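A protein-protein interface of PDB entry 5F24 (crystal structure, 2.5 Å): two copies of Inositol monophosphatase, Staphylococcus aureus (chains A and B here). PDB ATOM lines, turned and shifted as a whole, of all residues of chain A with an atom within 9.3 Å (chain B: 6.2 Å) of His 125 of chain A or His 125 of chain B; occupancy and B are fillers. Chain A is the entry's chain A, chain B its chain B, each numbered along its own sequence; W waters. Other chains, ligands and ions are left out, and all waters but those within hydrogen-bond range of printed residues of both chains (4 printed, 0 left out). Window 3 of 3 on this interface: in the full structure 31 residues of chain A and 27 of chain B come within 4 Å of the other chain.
Among the printed residues, merely in contact across the chains: His 125 of chain A with His 125 of chain B (3.7 Å).
Hydrophobic or aromatic side chains of chain B within 4 Å of the printed part of chain A: His 125.
Of the 22 printed residues of chain A, 5 touch a printed residue of chain B.
Hydrophobic or aromatic side chains of chain A within 4 Å of the printed part of chain B: His 125.
Among the printed residues, 6 pairs touch across the chains.
Among the printed residues, Asp or Glu carboxylates within 4 Å of a Lys or Arg side-chain nitrogen of the other chain: Glu 101 of chain A with Arg 191 of chain B, Asp 102 of chain A with Arg 191 of chain B, Arg 191 of chain A with Glu 101 of chain B and Arg 191 of chain A with Asp 102 of chain B.
Glu 101 of chain A touches Arg 191 of chain B, and with the chains exchanged Arg 191 of chain A touches Glu 101 of chain B.
Asp 102 of chain A touches Arg 191 of chain B, and with the chains exchanged Arg 191 of chain A touches Asp 102 of chain B.
His 125 of chain B touches its own counterpart, His 125 of chain A.
Positions printed for both chains: 101, 102, 122, 123, 124, 125, 126, 127, 140 and 191.
Of the 6 pairs that touch across the chains among the printed residues, 5 have their exchanged pair printed and touching as well.
The side-chain carboxylate (OE2) of Glu 101 of chain A lies within salt-bridge range of the guanidinium group (NH2) of Arg 191 of chain B, 3.7 Å away.
The side-chain carboxylate (OD2) of Asp 102 of chain B is in salt-bridge range of the guanidinium group (NH1) of Arg 191 of chain A.
The side-chain carboxylate (OE1) of Glu 101 of chain B sits at hydrogen-bond distance from the side-chain amide nitrogen (NE2) of Gln 196 of chain A (3.1 Å).
The side-chain carboxylate (OE2) of Glu 101 of chain B lies within salt-bridge range of the guanidinium group (NH2) of Arg 191 of chain A.
The side-chain carboxylate (OD2) of Asp 102 of chain A lies within salt-bridge range of the guanidinium group (NH1) of Arg 191 of chain B, at 2.7 Å.
Of the printed residues of chain B, Asp 102 of chain A touches Arg 191 (2.7 Å).
Of chain B, only His 125 comes within 4 Å of His 125 of chain A.
Tyr 129 of chain A touches none of the printed residues of chain B.
Val 182 of chain A touches none of the printed residues of chain B.
Printed residues of chain B within 4 Å of Arg 191 of chain A: Glu 101 and Asp 102.
Of the printed residues of chain B, Gln 196 of chain A touches Glu 101.
Of the printed residues of chain A, Asp 102 of chain B touches Arg 191 (2.8 Å).
His 125 of chain B touches just one residue of chain A: His 125 (3.7 Å).
The nearest residue of chain B that does not touch His 125 of chain A is Glu 101 of chain B (4.8 Å).
NE2 of His 125 of chain A sits at hydrogen-bond distance from OE2 of Glu 101 of chain A (3.2 Å).
OD2 of Asp 122 of chain B sits at hydrogen-bond distance from ND1 of His 125 of chain B, 2.8 Å away.
The side-chain amino group (NZ) of Lys 194 of chain A is in hydrogen-bond range of the side-chain amide oxygen (OE1) of Gln 196 of chain A (2.7 Å).
The backbone NH (N) of Gln 196 of chain A sits at hydrogen-bond distance from the backbone carbonyl oxygen (O) of Arg 191 of chain A (2.8 Å).
The side-chain carboxylate (OD2) of Asp 122 of chain A lies within hydrogen-bond range of a ring nitrogen (ND1) of His 125 of chain A (2.8 Å).
A ring nitrogen (NE2) of His 125 of chain B is in hydrogen-bond range of the side-chain carboxylate (OE2) of Glu 101 of chain B (3.3 Å).
Water W2 lies within hydrogen-bond range of NZ of Lys 194 of chain A (2.5 Å), OE1 of Glu 101 of chain B (3.2 Å) and OH of Tyr 129 of chain A (3.4 Å).
Water W1 lies within hydrogen-bond range of OE1 of Glu 101 of chain B, NZ of Lys 194 of chain A and NE of Arg 191 of chain A.
Water W3 lies within hydrogen-bond range of OD2 of Asp 102 of chain A (2.9 Å), O of Val 182 of chain A (3.0 Å) and NH1 of Arg 191 of chain B (3.2 Å).
Water W4 lies within hydrogen-bond range of the side-chain carboxylate (OD2) of Asp 102 of chain B (2.9 Å) and the guanidinium group (NH1) of Arg 191 of chain A (3.5 Å).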
ATOM      1  N   ASP A  21      21.018  18.333 -16.608  1.00  0.00           N
ATOM      2  CA  ASP A  21      19.964  17.679 -17.423  1.00  0.00           C
ATOM      3  C   ASP A  21      20.149  17.816 -18.915  1.00  0.00           C
ATOM      4  O   ASP A  21      19.624  17.013 -19.680  1.00  0.00           O
ATOM      5  CB  ASP A  21      18.559  18.261 -17.068  1.00  0.00           C
ATOM      6  CG  ASP A  21      18.274  18.281 -15.538  1.00  0.00           C
ATOM      7  OD1 ASP A  21      18.842  17.472 -14.791  1.00  0.00           O
ATOM      8  OD2 ASP A  21      17.503  19.137 -15.067  1.00  0.00           O
ATOM      9  N   GLN A 100      20.048   2.045 -16.351  1.00  0.00           N
ATOM     10  CA  GLN A 100      19.758   3.471 -16.672  1.00  0.00           C
ATOM     11  C   GLN A 100      18.684   4.046 -15.794  1.00  0.00           C
ATOM     12  O   GLN A 100      17.891   4.882 -16.223  1.00  0.00           O
ATOM     13  CB  GLN A 100      19.315   3.596 -18.092  1.00  0.00           C
ATOM     14  CG  GLN A 100      20.485   3.698 -18.988  1.00  0.00           C
ATOM     15  CD  GLN A 100      20.408   2.718 -20.100  1.00  0.00           C
ATOM     16  OE1 GLN A 100      20.099   1.512 -19.890  1.00  0.00           O
ATOM     17  NE2 GLN A 100      20.714   3.204 -21.300  1.00  0.00           N
ATOM     18  N   GLU A 101      18.687   3.621 -14.545  1.00  0.00           N
ATOM     19  CA  GLU A 101      17.745   4.089 -13.560  1.00  0.00           C
ATOM     20  C   GLU A 101      18.363   3.840 -12.227  1.00  0.00           C
ATOM     21  O   GLU A 101      19.250   3.002 -12.042  1.00  0.00           O
ATOM     22  CB  GLU A 101      16.413   3.362 -13.815  1.00  0.00           C
ATOM     23  CG  GLU A 101      15.357   3.701 -12.784  1.00  0.00           C
ATOM     24  CD  GLU A 101      13.945   3.177 -13.099  1.00  0.00           C
ATOM     25  OE1 GLU A 101      13.725   2.479 -14.126  1.00  0.00           O
ATOM     26  OE2 GLU A 101      13.071   3.507 -12.257  1.00  0.00           O
ATOM     27  N   ASP A 102      17.854   4.507 -11.208  1.00  0.00           N
ATOM     28  CA  ASP A 102      18.283   4.234  -9.796  1.00  0.00           C
ATOM     29  C   ASP A 102      19.741   4.563  -9.544  1.00  0.00           C
ATOM     30  O   ASP A 102      20.514   3.785  -8.945  1.00  0.00           O
ATOM     31  CB  ASP A 102      17.989   2.770  -9.347  1.00  0.00           C
ATOM     32  CG  ASP A 102      16.511   2.474  -9.284  1.00  0.00           C
ATOM     33  OD1 ASP A 102      15.741   3.434  -9.102  1.00  0.00           O
ATOM     34  OD2 ASP A 102      16.104   1.285  -9.400  1.00  0.00           O
ATOM     35  N   TYR A 103      20.105   5.755 -10.006  1.00  0.00           N
ATOM     36  CA  TYR A 103      21.417   6.297  -9.689  1.00  0.00           C
ATOM     37  C   TYR A 103      21.236   7.787  -9.348  1.00  0.00           C
ATOM     38  O   TYR A 103      20.145   8.349  -9.581  1.00  0.00           O
ATOM     39  CB  TYR A 103      22.353   6.094 -10.870  1.00  0.00           C
ATOM     40  CG  TYR A 103      21.889   6.752 -12.133  1.00  0.00           C
ATOM     41  CD1 TYR A 103      22.206   8.076 -12.395  1.00  0.00           C
ATOM     42  CD2 TYR A 103      21.182   6.033 -13.106  1.00  0.00           C
ATOM     43  CE1 TYR A 103      21.810   8.668 -13.573  1.00  0.00           C
ATOM     44  CE2 TYR A 103      20.766   6.634 -14.278  1.00  0.00           C
ATOM     45  CZ  TYR A 103      21.090   7.942 -14.497  1.00  0.00           C
ATOM     46  OH  TYR A 103      20.705   8.563 -15.640  1.00  0.00           O
ATOM     47  N   CYS A 104      22.263   8.403  -8.765  1.00  0.00           N
ATOM     48  CA  CYS A 104      22.148   9.747  -8.319  1.00  0.00           C
ATOM     49  C   CYS A 104      23.481  10.462  -8.330  1.00  0.00           C
ATOM     50  O   CYS A 104      24.552   9.862  -8.444  1.00  0.00           O
ATOM     51  CB  CYS A 104      21.529   9.774  -6.918  1.00  0.00           C
ATOM     52  SG  CYS A 104      22.572   8.974  -5.652  1.00  0.00           S
ATOM     53  N   TYR A 121      20.738  14.013  -5.948  1.00  0.00           N
ATOM     54  CA  TYR A 121      19.911  14.293  -7.102  1.00  0.00           C
ATOM     55  C   TYR A 121      19.558  12.961  -7.786  1.00  0.00           C
ATOM     56  O   TYR A 121      20.404  12.309  -8.465  1.00  0.00           O
ATOM     57  CB  TYR A 121      20.624  15.236  -8.083  1.00  0.00           C
ATOM     58  CG  TYR A 121      19.758  15.633  -9.275  1.00  0.00           C
ATOM     59  CD1 TYR A 121      18.382  15.771  -9.150  1.00  0.00           C
ATOM     60  CD2 TYR A 121      20.323  15.854 -10.534  1.00  0.00           C
ATOM     61  CE1 TYR A 121      17.596  16.120 -10.228  1.00  0.00           C
ATOM     62  CE2 TYR A 121      19.531  16.242 -11.637  1.00  0.00           C
ATOM     63  CZ  TYR A 121      18.176  16.345 -11.468  1.00  0.00           C
ATOM     64  OH  TYR A 121      17.400  16.684 -12.502  1.00  0.00           O
ATOM     65  N   ASP A 122      18.301  12.582  -7.599  1.00  0.00           N
ATOM     66  CA  ASP A 122      17.797  11.355  -8.282  1.00  0.00           C
ATOM     67  C   ASP A 122      17.404  11.754  -9.660  1.00  0.00           C
ATOM     68  O   ASP A 122      16.251  12.158  -9.883  1.00  0.00           O
ATOM     69  CB  ASP A 122      16.602  10.769  -7.543  1.00  0.00           C
ATOM     70  CG  ASP A 122      15.947   9.609  -8.278  1.00  0.00           C
ATOM     71  OD1 ASP A 122      16.222   9.397  -9.479  1.00  0.00           O
ATOM     72  OD2 ASP A 122      15.124   8.925  -7.641  1.00  0.00           O
ATOM     73  N   TYR A 123      18.361  11.698 -10.572  1.00  0.00           N
ATOM     74  CA  TYR A 123      18.146  12.299 -11.874  1.00  0.00           C
ATOM     75  C   TYR A 123      17.106  11.529 -12.708  1.00  0.00           C
ATOM     76  O   TYR A 123      16.248  12.151 -13.340  1.00  0.00           O
ATOM     77  CB  TYR A 123      19.484  12.390 -12.664  1.00  0.00           C
ATOM     78  CG  TYR A 123      19.310  12.607 -14.164  1.00  0.00           C
ATOM     79  CD1 TYR A 123      19.094  13.873 -14.693  1.00  0.00           C
ATOM     80  CD2 TYR A 123      19.342  11.539 -15.039  1.00  0.00           C
ATOM     81  CE1 TYR A 123      18.931  14.068 -16.060  1.00  0.00           C
ATOM     82  CE2 TYR A 123      19.165  11.704 -16.389  1.00  0.00           C
ATOM     83  CZ  TYR A 123      18.976  12.972 -16.893  1.00  0.00           C
ATOM     84  OH  TYR A 123      18.823  13.130 -18.238  1.00  0.00           O
ATOM     85  N   PRO A 124      17.145  10.199 -12.715  1.00  0.00           N
ATOM     86  CA  PRO A 124      16.136   9.458 -13.542  1.00  0.00           C
ATOM     87  C   PRO A 124      14.713   9.844 -13.186  1.00  0.00           C
ATOM     88  O   PRO A 124      13.823   9.799 -14.027  1.00  0.00           O
ATOM     89  CB  PRO A 124      16.408   7.996 -13.215  1.00  0.00           C
ATOM     90  CG  PRO A 124      17.836   7.985 -12.786  1.00  0.00           C
ATOM     91  CD  PRO A 124      18.132   9.295 -12.125  1.00  0.00           C
ATOM     92  N   HIS A 125      14.485  10.197 -11.935  1.00  0.00           N
ATOM     93  CA  HIS A 125      13.095  10.538 -11.506  1.00  0.00           C
ATOM     94  C   HIS A 125      12.937  11.993 -11.324  1.00  0.00           C
ATOM     95  O   HIS A 125      11.857  12.379 -10.798  1.00  0.00           O
ATOM     96  CB  HIS A 125      12.674   9.886 -10.182  1.00  0.00           C
ATOM     97  CG  HIS A 125      12.660   8.408 -10.240  1.00  0.00           C
ATOM     98  ND1 HIS A 125      13.253   7.622  -9.279  1.00  0.00           N
ATOM     99  CD2 HIS A 125      12.210   7.564 -11.196  1.00  0.00           C
ATOM    100  CE1 HIS A 125      13.134   6.353  -9.626  1.00  0.00           C
ATOM    101  NE2 HIS A 125      12.514   6.290 -10.790  1.00  0.00           N
ATOM    102  N   LYS A 126      13.942  12.806 -11.688  1.00  0.00           N
ATOM    103  CA  LYS A 126      13.910  14.259 -11.464  1.00  0.00           C
ATOM    104  C   LYS A 126      13.477  14.647 -10.037  1.00  0.00           C
ATOM    105  O   LYS A 126      12.587  15.456  -9.854  1.00  0.00           O
ATOM    106  CB  LYS A 126      12.948  14.874 -12.493  1.00  0.00           C
ATOM    107  CG  LYS A 126      13.320  14.592 -13.952  1.00  0.00           C
ATOM    108  CD  LYS A 126      14.633  15.312 -14.313  1.00  0.00           C
ATOM    109  CE  LYS A 126      15.062  15.080 -15.766  1.00  0.00           C
ATOM    110  NZ  LYS A 126      15.508  13.672 -15.955  1.00  0.00           N
ATOM    111  N   LYS A 127      14.092  14.046  -9.039  1.00  0.00           N
ATOM    112  CA  LYS A 127      13.803  14.369  -7.686  1.00  0.00           C
ATOM    113  C   LYS A 127      15.097  14.846  -7.029  1.00  0.00           C
ATOM    114  O   LYS A 127      16.076  14.063  -6.882  1.00  0.00           O
ATOM    115  CB  LYS A 127      13.229  13.195  -6.913  1.00  0.00           C
ATOM    116  CG  LYS A 127      11.797  12.928  -7.306  1.00  0.00           C
ATOM    117  CD  LYS A 127      11.106  12.005  -6.338  1.00  0.00           C
ATOM    118  CE  LYS A 127       9.612  12.143  -6.486  1.00  0.00           C
ATOM    119  NZ  LYS A 127       8.965  10.883  -6.011  1.00  0.00           N
ATOM    120  N   LEU A 128      15.114  16.099  -6.643  1.00  0.00           N
ATOM    121  CA  LEU A 128      16.263  16.719  -5.952  1.00  0.00           C
ATOM    122  C   LEU A 128      16.042  16.765  -4.437  1.00  0.00           C
ATOM    123  O   LEU A 128      15.137  17.452  -3.989  1.00  0.00           O
ATOM    124  CB  LEU A 128      16.553  18.106  -6.489  1.00  0.00           C
ATOM    125  CG  LEU A 128      17.707  18.810  -5.795  1.00  0.00           C
ATOM    126  CD1 LEU A 128      18.997  18.016  -5.945  1.00  0.00           C
ATOM    127  CD2 LEU A 128      17.880  20.213  -6.390  1.00  0.00           C
ATOM    128  N   TYR A 129      16.809  15.957  -3.710  1.00  0.00           N
ATOM    129  CA  TYR A 129      16.724  15.981  -2.274  1.00  0.00           C
ATOM    130  C   TYR A 129      17.823  16.934  -1.853  1.00  0.00           C
ATOM    131  O   TYR A 129      18.949  16.858  -2.361  1.00  0.00           O
ATOM    132  CB  TYR A 129      16.979  14.636  -1.668  1.00  0.00           C
ATOM    133  CG  TYR A 129      15.992  13.617  -2.104  1.00  0.00           C
ATOM    134  CD1 TYR A 129      14.745  13.517  -1.496  1.00  0.00           C
ATOM    135  CD2 TYR A 129      16.276  12.753  -3.133  1.00  0.00           C
ATOM    136  CE1 TYR A 129      13.819  12.553  -1.891  1.00  0.00           C
ATOM    137  CE2 TYR A 129      15.348  11.805  -3.550  1.00  0.00           C
ATOM    138  CZ  TYR A 129      14.120  11.714  -2.919  1.00  0.00           C
ATOM    139  OH  TYR A 129      13.227  10.815  -3.375  1.00  0.00           O
ATOM    140  N   CYS A 139      12.457  17.985  -0.822  1.00  0.00           N
ATOM    141  CA  CYS A 139      12.411  17.185  -2.040  1.00  0.00           C
ATOM    142  C   CYS A 139      11.736  18.003  -3.101  1.00  0.00           C
ATOM    143  O   CYS A 139      10.530  18.231  -3.010  1.00  0.00           O
ATOM    144  CB  CYS A 139      11.631  15.911  -1.758  1.00  0.00           C
ATOM    145  SG  CYS A 139      11.667  14.829  -3.188  1.00  0.00           S
ATOM    146  N   ASN A 140      12.483  18.434  -4.113  1.00  0.00           N
ATOM    147  CA  ASN A 140      11.923  19.314  -5.160  1.00  0.00           C
ATOM    148  C   ASN A 140      11.170  20.484  -4.514  1.00  0.00           C
ATOM    149  O   ASN A 140      10.074  20.823  -4.917  1.00  0.00           O
ATOM    150  CB  ASN A 140      10.951  18.559  -6.085  1.00  0.00           C
ATOM    151  CG  ASN A 140      11.659  17.709  -7.103  1.00  0.00           C
ATOM    152  OD1 ASN A 140      12.885  17.823  -7.308  1.00  0.00           O
ATOM    153  ND2 ASN A 140      10.920  16.818  -7.725  1.00  0.00           N
ATOM    154  N   VAL A 182      17.517  -0.706  -3.345  1.00  0.00           N
ATOM    155  CA  VAL A 182      17.566   0.150  -4.520  1.00  0.00           C
ATOM    156  C   VAL A 182      18.913   0.025  -5.215  1.00  0.00           C
ATOM    157  O   VAL A 182      18.976  -0.014  -6.423  1.00  0.00           O
ATOM    158  CB  VAL A 182      17.299   1.611  -4.191  1.00  0.00           C
ATOM    159  CG1 VAL A 182      17.376   2.452  -5.454  1.00  0.00           C
ATOM    160  CG2 VAL A 182      15.927   1.763  -3.554  1.00  0.00           C
ATOM    161  N   LEU A 187      20.439   6.758  -2.595  1.00  0.00           N
ATOM    162  CA  LEU A 187      18.978   6.613  -2.754  1.00  0.00           C
ATOM    163  C   LEU A 187      18.415   5.728  -1.656  1.00  0.00           C
ATOM    164  O   LEU A 187      17.383   6.038  -1.065  1.00  0.00           O
ATOM    165  CB  LEU A 187      18.662   6.065  -4.118  1.00  0.00           C
ATOM    166  CG  LEU A 187      19.113   6.964  -5.283  1.00  0.00           C
ATOM    167  CD1 LEU A 187      18.841   6.270  -6.621  1.00  0.00           C
ATOM    168  CD2 LEU A 187      18.410   8.307  -5.272  1.00  0.00           C
ATOM    169  N   ARG A 191      15.634   6.901   1.191  1.00  0.00           N
ATOM    170  CA  ARG A 191      14.439   6.181   1.616  1.00  0.00           C
ATOM    171  C   ARG A 191      14.294   6.112   3.153  1.00  0.00           C
ATOM    172  O   ARG A 191      13.166   6.195   3.709  1.00  0.00           O
ATOM    173  CB  ARG A 191      14.388   4.765   1.064  1.00  0.00           C
ATOM    174  CG  ARG A 191      14.376   4.781  -0.448  1.00  0.00           C
ATOM    175  CD  ARG A 191      13.374   3.850  -1.050  1.00  0.00           C
ATOM    176  NE  ARG A 191      13.324   4.034  -2.476  1.00  0.00           N
ATOM    177  CZ  ARG A 191      12.559   3.305  -3.291  1.00  0.00           C
ATOM    178  NH1 ARG A 191      11.756   2.369  -2.816  1.00  0.00           N
ATOM    179  NH2 ARG A 191      12.579   3.518  -4.585  1.00  0.00           N
ATOM    180  N   LYS A 194      13.045   9.568   4.173  1.00  0.00           N
ATOM    181  CA  LYS A 194      11.633   9.771   3.839  1.00  0.00           C
ATOM    182  C   LYS A 194      10.731   8.928   4.728  1.00  0.00           C
ATOM    183  O   LYS A 194       9.526   9.066   4.671  1.00  0.00           O
ATOM    184  CB  LYS A 194      11.379   9.448   2.374  1.00  0.00           C
ATOM    185  CG  LYS A 194      11.853  10.536   1.434  1.00  0.00           C
ATOM    186  CD  LYS A 194      11.614  10.120  -0.014  1.00  0.00           C
ATOM    187  CE  LYS A 194      12.799   9.294  -0.502  1.00  0.00           C
ATOM    188  NZ  LYS A 194      12.483   8.493  -1.737  1.00  0.00           N
ATOM    189  N   GLN A 196      10.488   5.636   4.349  1.00  0.00           N
ATOM    190  CA  GLN A 196      10.124   4.474   3.561  1.00  0.00           C
ATOM    191  C   GLN A 196      10.851   3.207   4.008  1.00  0.00           C
ATOM    192  O   GLN A 196      10.303   2.106   3.947  1.00  0.00           O
ATOM    193  CB  GLN A 196      10.372   4.758   2.080  1.00  0.00           C
ATOM    194  CG  GLN A 196       9.621   5.971   1.504  1.00  0.00           C
ATOM    195  CD  GLN A 196      10.071   6.285   0.060  1.00  0.00           C
ATOM    196  OE1 GLN A 196      11.212   6.676  -0.172  1.00  0.00           O
ATOM    197  NE2 GLN A 196       9.198   6.118  -0.886  1.00  0.00           N
ATOM    198  N   GLU B 101       5.242   3.828  -2.761  1.00  0.00           N
ATOM    199  CA  GLU B 101       5.962   3.842  -3.991  1.00  0.00           C
ATOM    200  C   GLU B 101       6.224   2.392  -4.318  1.00  0.00           C
ATOM    201  O   GLU B 101       6.129   1.524  -3.450  1.00  0.00           O
ATOM    202  CB  GLU B 101       7.233   4.684  -3.812  1.00  0.00           C
ATOM    203  CG  GLU B 101       8.134   4.652  -5.037  1.00  0.00           C
ATOM    204  CD  GLU B 101       9.338   5.587  -4.977  1.00  0.00           C
ATOM    205  OE1 GLU B 101       9.547   6.311  -3.959  1.00  0.00           O
ATOM    206  OE2 GLU B 101      10.069   5.552  -6.002  1.00  0.00           O
ATOM    207  N   ASP B 102       6.570   2.121  -5.568  1.00  0.00           N
ATOM    208  CA  ASP B 102       6.919   0.741  -5.992  1.00  0.00           C
ATOM    209  C   ASP B 102       5.790  -0.288  -5.826  1.00  0.00           C
ATOM    210  O   ASP B 102       5.975  -1.389  -5.307  1.00  0.00           O
ATOM    211  CB  ASP B 102       8.192   0.242  -5.287  1.00  0.00           C
ATOM    212  CG  ASP B 102       9.416   1.026  -5.687  1.00  0.00           C
ATOM    213  OD1 ASP B 102       9.413   1.583  -6.783  1.00  0.00           O
ATOM    214  OD2 ASP B 102      10.373   1.109  -4.896  1.00  0.00           O
ATOM    215  N   ASP B 122       2.535   1.121 -13.467  1.00  0.00           N
ATOM    216  CA  ASP B 122       3.373   1.617 -12.354  1.00  0.00           C
ATOM    217  C   ASP B 122       2.857   3.002 -12.007  1.00  0.00           C
ATOM    218  O   ASP B 122       3.334   3.995 -12.560  1.00  0.00           O
ATOM    219  CB  ASP B 122       4.828   1.706 -12.790  1.00  0.00           C
ATOM    220  CG  ASP B 122       5.723   2.378 -11.772  1.00  0.00           C
ATOM    221  OD1 ASP B 122       5.222   2.990 -10.797  1.00  0.00           O
ATOM    222  OD2 ASP B 122       6.966   2.267 -11.940  1.00  0.00           O
ATOM    223  N   TYR B 123       1.882   3.053 -11.108  1.00  0.00           N
ATOM    224  CA  TYR B 123       1.158   4.286 -10.893  1.00  0.00           C
ATOM    225  C   TYR B 123       2.012   5.367 -10.225  1.00  0.00           C
ATOM    226  O   TYR B 123       1.983   6.522 -10.635  1.00  0.00           O
ATOM    227  CB  TYR B 123      -0.097   4.017 -10.018  1.00  0.00           C
ATOM    228  CG  TYR B 123      -0.692   5.242  -9.398  1.00  0.00           C
ATOM    229  CD1 TYR B 123      -1.554   6.076 -10.120  1.00  0.00           C
ATOM    230  CD2 TYR B 123      -0.404   5.583  -8.090  1.00  0.00           C
ATOM    231  CE1 TYR B 123      -2.082   7.212  -9.553  1.00  0.00           C
ATOM    232  CE2 TYR B 123      -0.920   6.728  -7.513  1.00  0.00           C
ATOM    233  CZ  TYR B 123      -1.751   7.543  -8.246  1.00  0.00           C
ATOM    234  OH  TYR B 123      -2.228   8.696  -7.647  1.00  0.00           O
ATOM    235  N   PRO B 124       2.879   5.016  -9.250  1.00  0.00           N
ATOM    236  CA  PRO B 124       3.698   6.060  -8.595  1.00  0.00           C
ATOM    237  C   PRO B 124       4.562   6.758  -9.603  1.00  0.00           C
ATOM    238  O   PRO B 124       4.870   7.956  -9.408  1.00  0.00           O
ATOM    239  CB  PRO B 124       4.559   5.295  -7.600  1.00  0.00           C
ATOM    240  CG  PRO B 124       3.751   4.103  -7.289  1.00  0.00           C
ATOM    241  CD  PRO B 124       2.999   3.742  -8.532  1.00  0.00           C
ATOM    242  N   HIS B 125       5.060   6.062 -10.628  1.00  0.00           N
ATOM    243  CA  HIS B 125       5.865   6.733 -11.643  1.00  0.00           C
ATOM    244  C   HIS B 125       5.113   7.116 -12.875  1.00  0.00           C
ATOM    245  O   HIS B 125       5.802   7.505 -13.836  1.00  0.00           O
ATOM    246  CB  HIS B 125       7.069   5.902 -12.066  1.00  0.00           C
ATOM    247  CG  HIS B 125       7.979   5.580 -10.944  1.00  0.00           C
ATOM    248  ND1 HIS B 125       8.469   4.313 -10.725  1.00  0.00           N
ATOM    249  CD2 HIS B 125       8.460   6.355  -9.943  1.00  0.00           C
ATOM    250  CE1 HIS B 125       9.233   4.324  -9.648  1.00  0.00           C
ATOM    251  NE2 HIS B 125       9.240   5.549  -9.150  1.00  0.00           N
ATOM    252  N   LYS B 126       3.776   6.947 -12.902  1.00  0.00           N
ATOM    253  CA  LYS B 126       2.988   7.139 -14.091  1.00  0.00           C
ATOM    254  C   LYS B 126       3.565   6.465 -15.349  1.00  0.00           C
ATOM    255  O   LYS B 126       3.729   7.112 -16.391  1.00  0.00           O
ATOM    256  CB  LYS B 126       2.872   8.666 -14.321  1.00  0.00           C
ATOM    257  CG  LYS B 126       2.233   9.431 -13.156  1.00  0.00           C
ATOM    258  CD  LYS B 126       0.751   9.046 -13.023  1.00  0.00           C
ATOM    259  CE  LYS B 126       0.059   9.770 -11.876  1.00  0.00           C
ATOM    260  NZ  LYS B 126       0.558   9.268 -10.559  1.00  0.00           N
ATOM    261  N   LYS B 127       3.910   5.188 -15.240  1.00  0.00           N
ATOM    262  CA  LYS B 127       4.424   4.446 -16.342  1.00  0.00           C
ATOM    263  C   LYS B 127       3.509   3.255 -16.621  1.00  0.00           C
ATOM    264  O   LYS B 127       3.365   2.359 -15.769  1.00  0.00           O
ATOM    265  CB  LYS B 127       5.847   4.009 -16.120  1.00  0.00           C
ATOM    266  CG  LYS B 127       6.810   5.163 -16.225  1.00  0.00           C
ATOM    267  CD  LYS B 127       8.221   4.678 -16.385  1.00  0.00           C
ATOM    268  CE  LYS B 127       9.092   5.791 -16.959  1.00  0.00           C
ATOM    269  NZ  LYS B 127      10.530   5.540 -16.575  1.00  0.00           N
ATOM    270  N   ASN B 140       3.973   3.710 -21.872  1.00  0.00           N
ATOM    271  CA  ASN B 140       3.357   5.032 -22.154  1.00  0.00           C
ATOM    272  C   ASN B 140       3.324   5.269 -23.655  1.00  0.00           C
ATOM    273  O   ASN B 140       3.646   6.354 -24.112  1.00  0.00           O
ATOM    274  CB  ASN B 140       4.140   6.176 -21.437  1.00  0.00           C
ATOM    275  CG  ASN B 140       3.921   6.188 -19.907  1.00  0.00           C
ATOM    276  OD1 ASN B 140       3.026   5.534 -19.394  1.00  0.00           O
ATOM    277  ND2 ASN B 140       4.745   6.906 -19.194  1.00  0.00           N
ATOM    278  N   ARG B 191      11.163  -5.071 -15.087  1.00  0.00           N
ATOM    279  CA  ARG B 191      12.600  -4.791 -15.217  1.00  0.00           C
ATOM    280  C   ARG B 191      13.282  -5.852 -16.095  1.00  0.00           C
ATOM    281  O   ARG B 191      14.244  -5.564 -16.840  1.00  0.00           O
ATOM    282  CB  ARG B 191      13.274  -4.709 -13.869  1.00  0.00           C
ATOM    283  CG  ARG B 191      12.686  -3.586 -13.036  1.00  0.00           C
ATOM    284  CD  ARG B 191      13.731  -2.737 -12.383  1.00  0.00           C
ATOM    285  NE  ARG B 191      13.136  -1.613 -11.699  1.00  0.00           N
ATOM    286  CZ  ARG B 191      13.830  -0.710 -11.005  1.00  0.00           C
ATOM    287  NH1 ARG B 191      15.142  -0.796 -10.896  1.00  0.00           N
ATOM    288  NH2 ARG B 191      13.221   0.308 -10.422  1.00  0.00           N
HETATM  289  O   HOH W   1      12.097   6.829  -3.818  1.00  0.00           O
HETATM  290  O   HOH W   2      10.316   9.232  -2.784  1.00  0.00           O
HETATM  291  O   HOH W   3      17.503  -1.129  -8.780  1.00  0.00           O
HETATM  292  O   HOH W   4      11.014  -1.029  -3.107  1.00  0.00           O
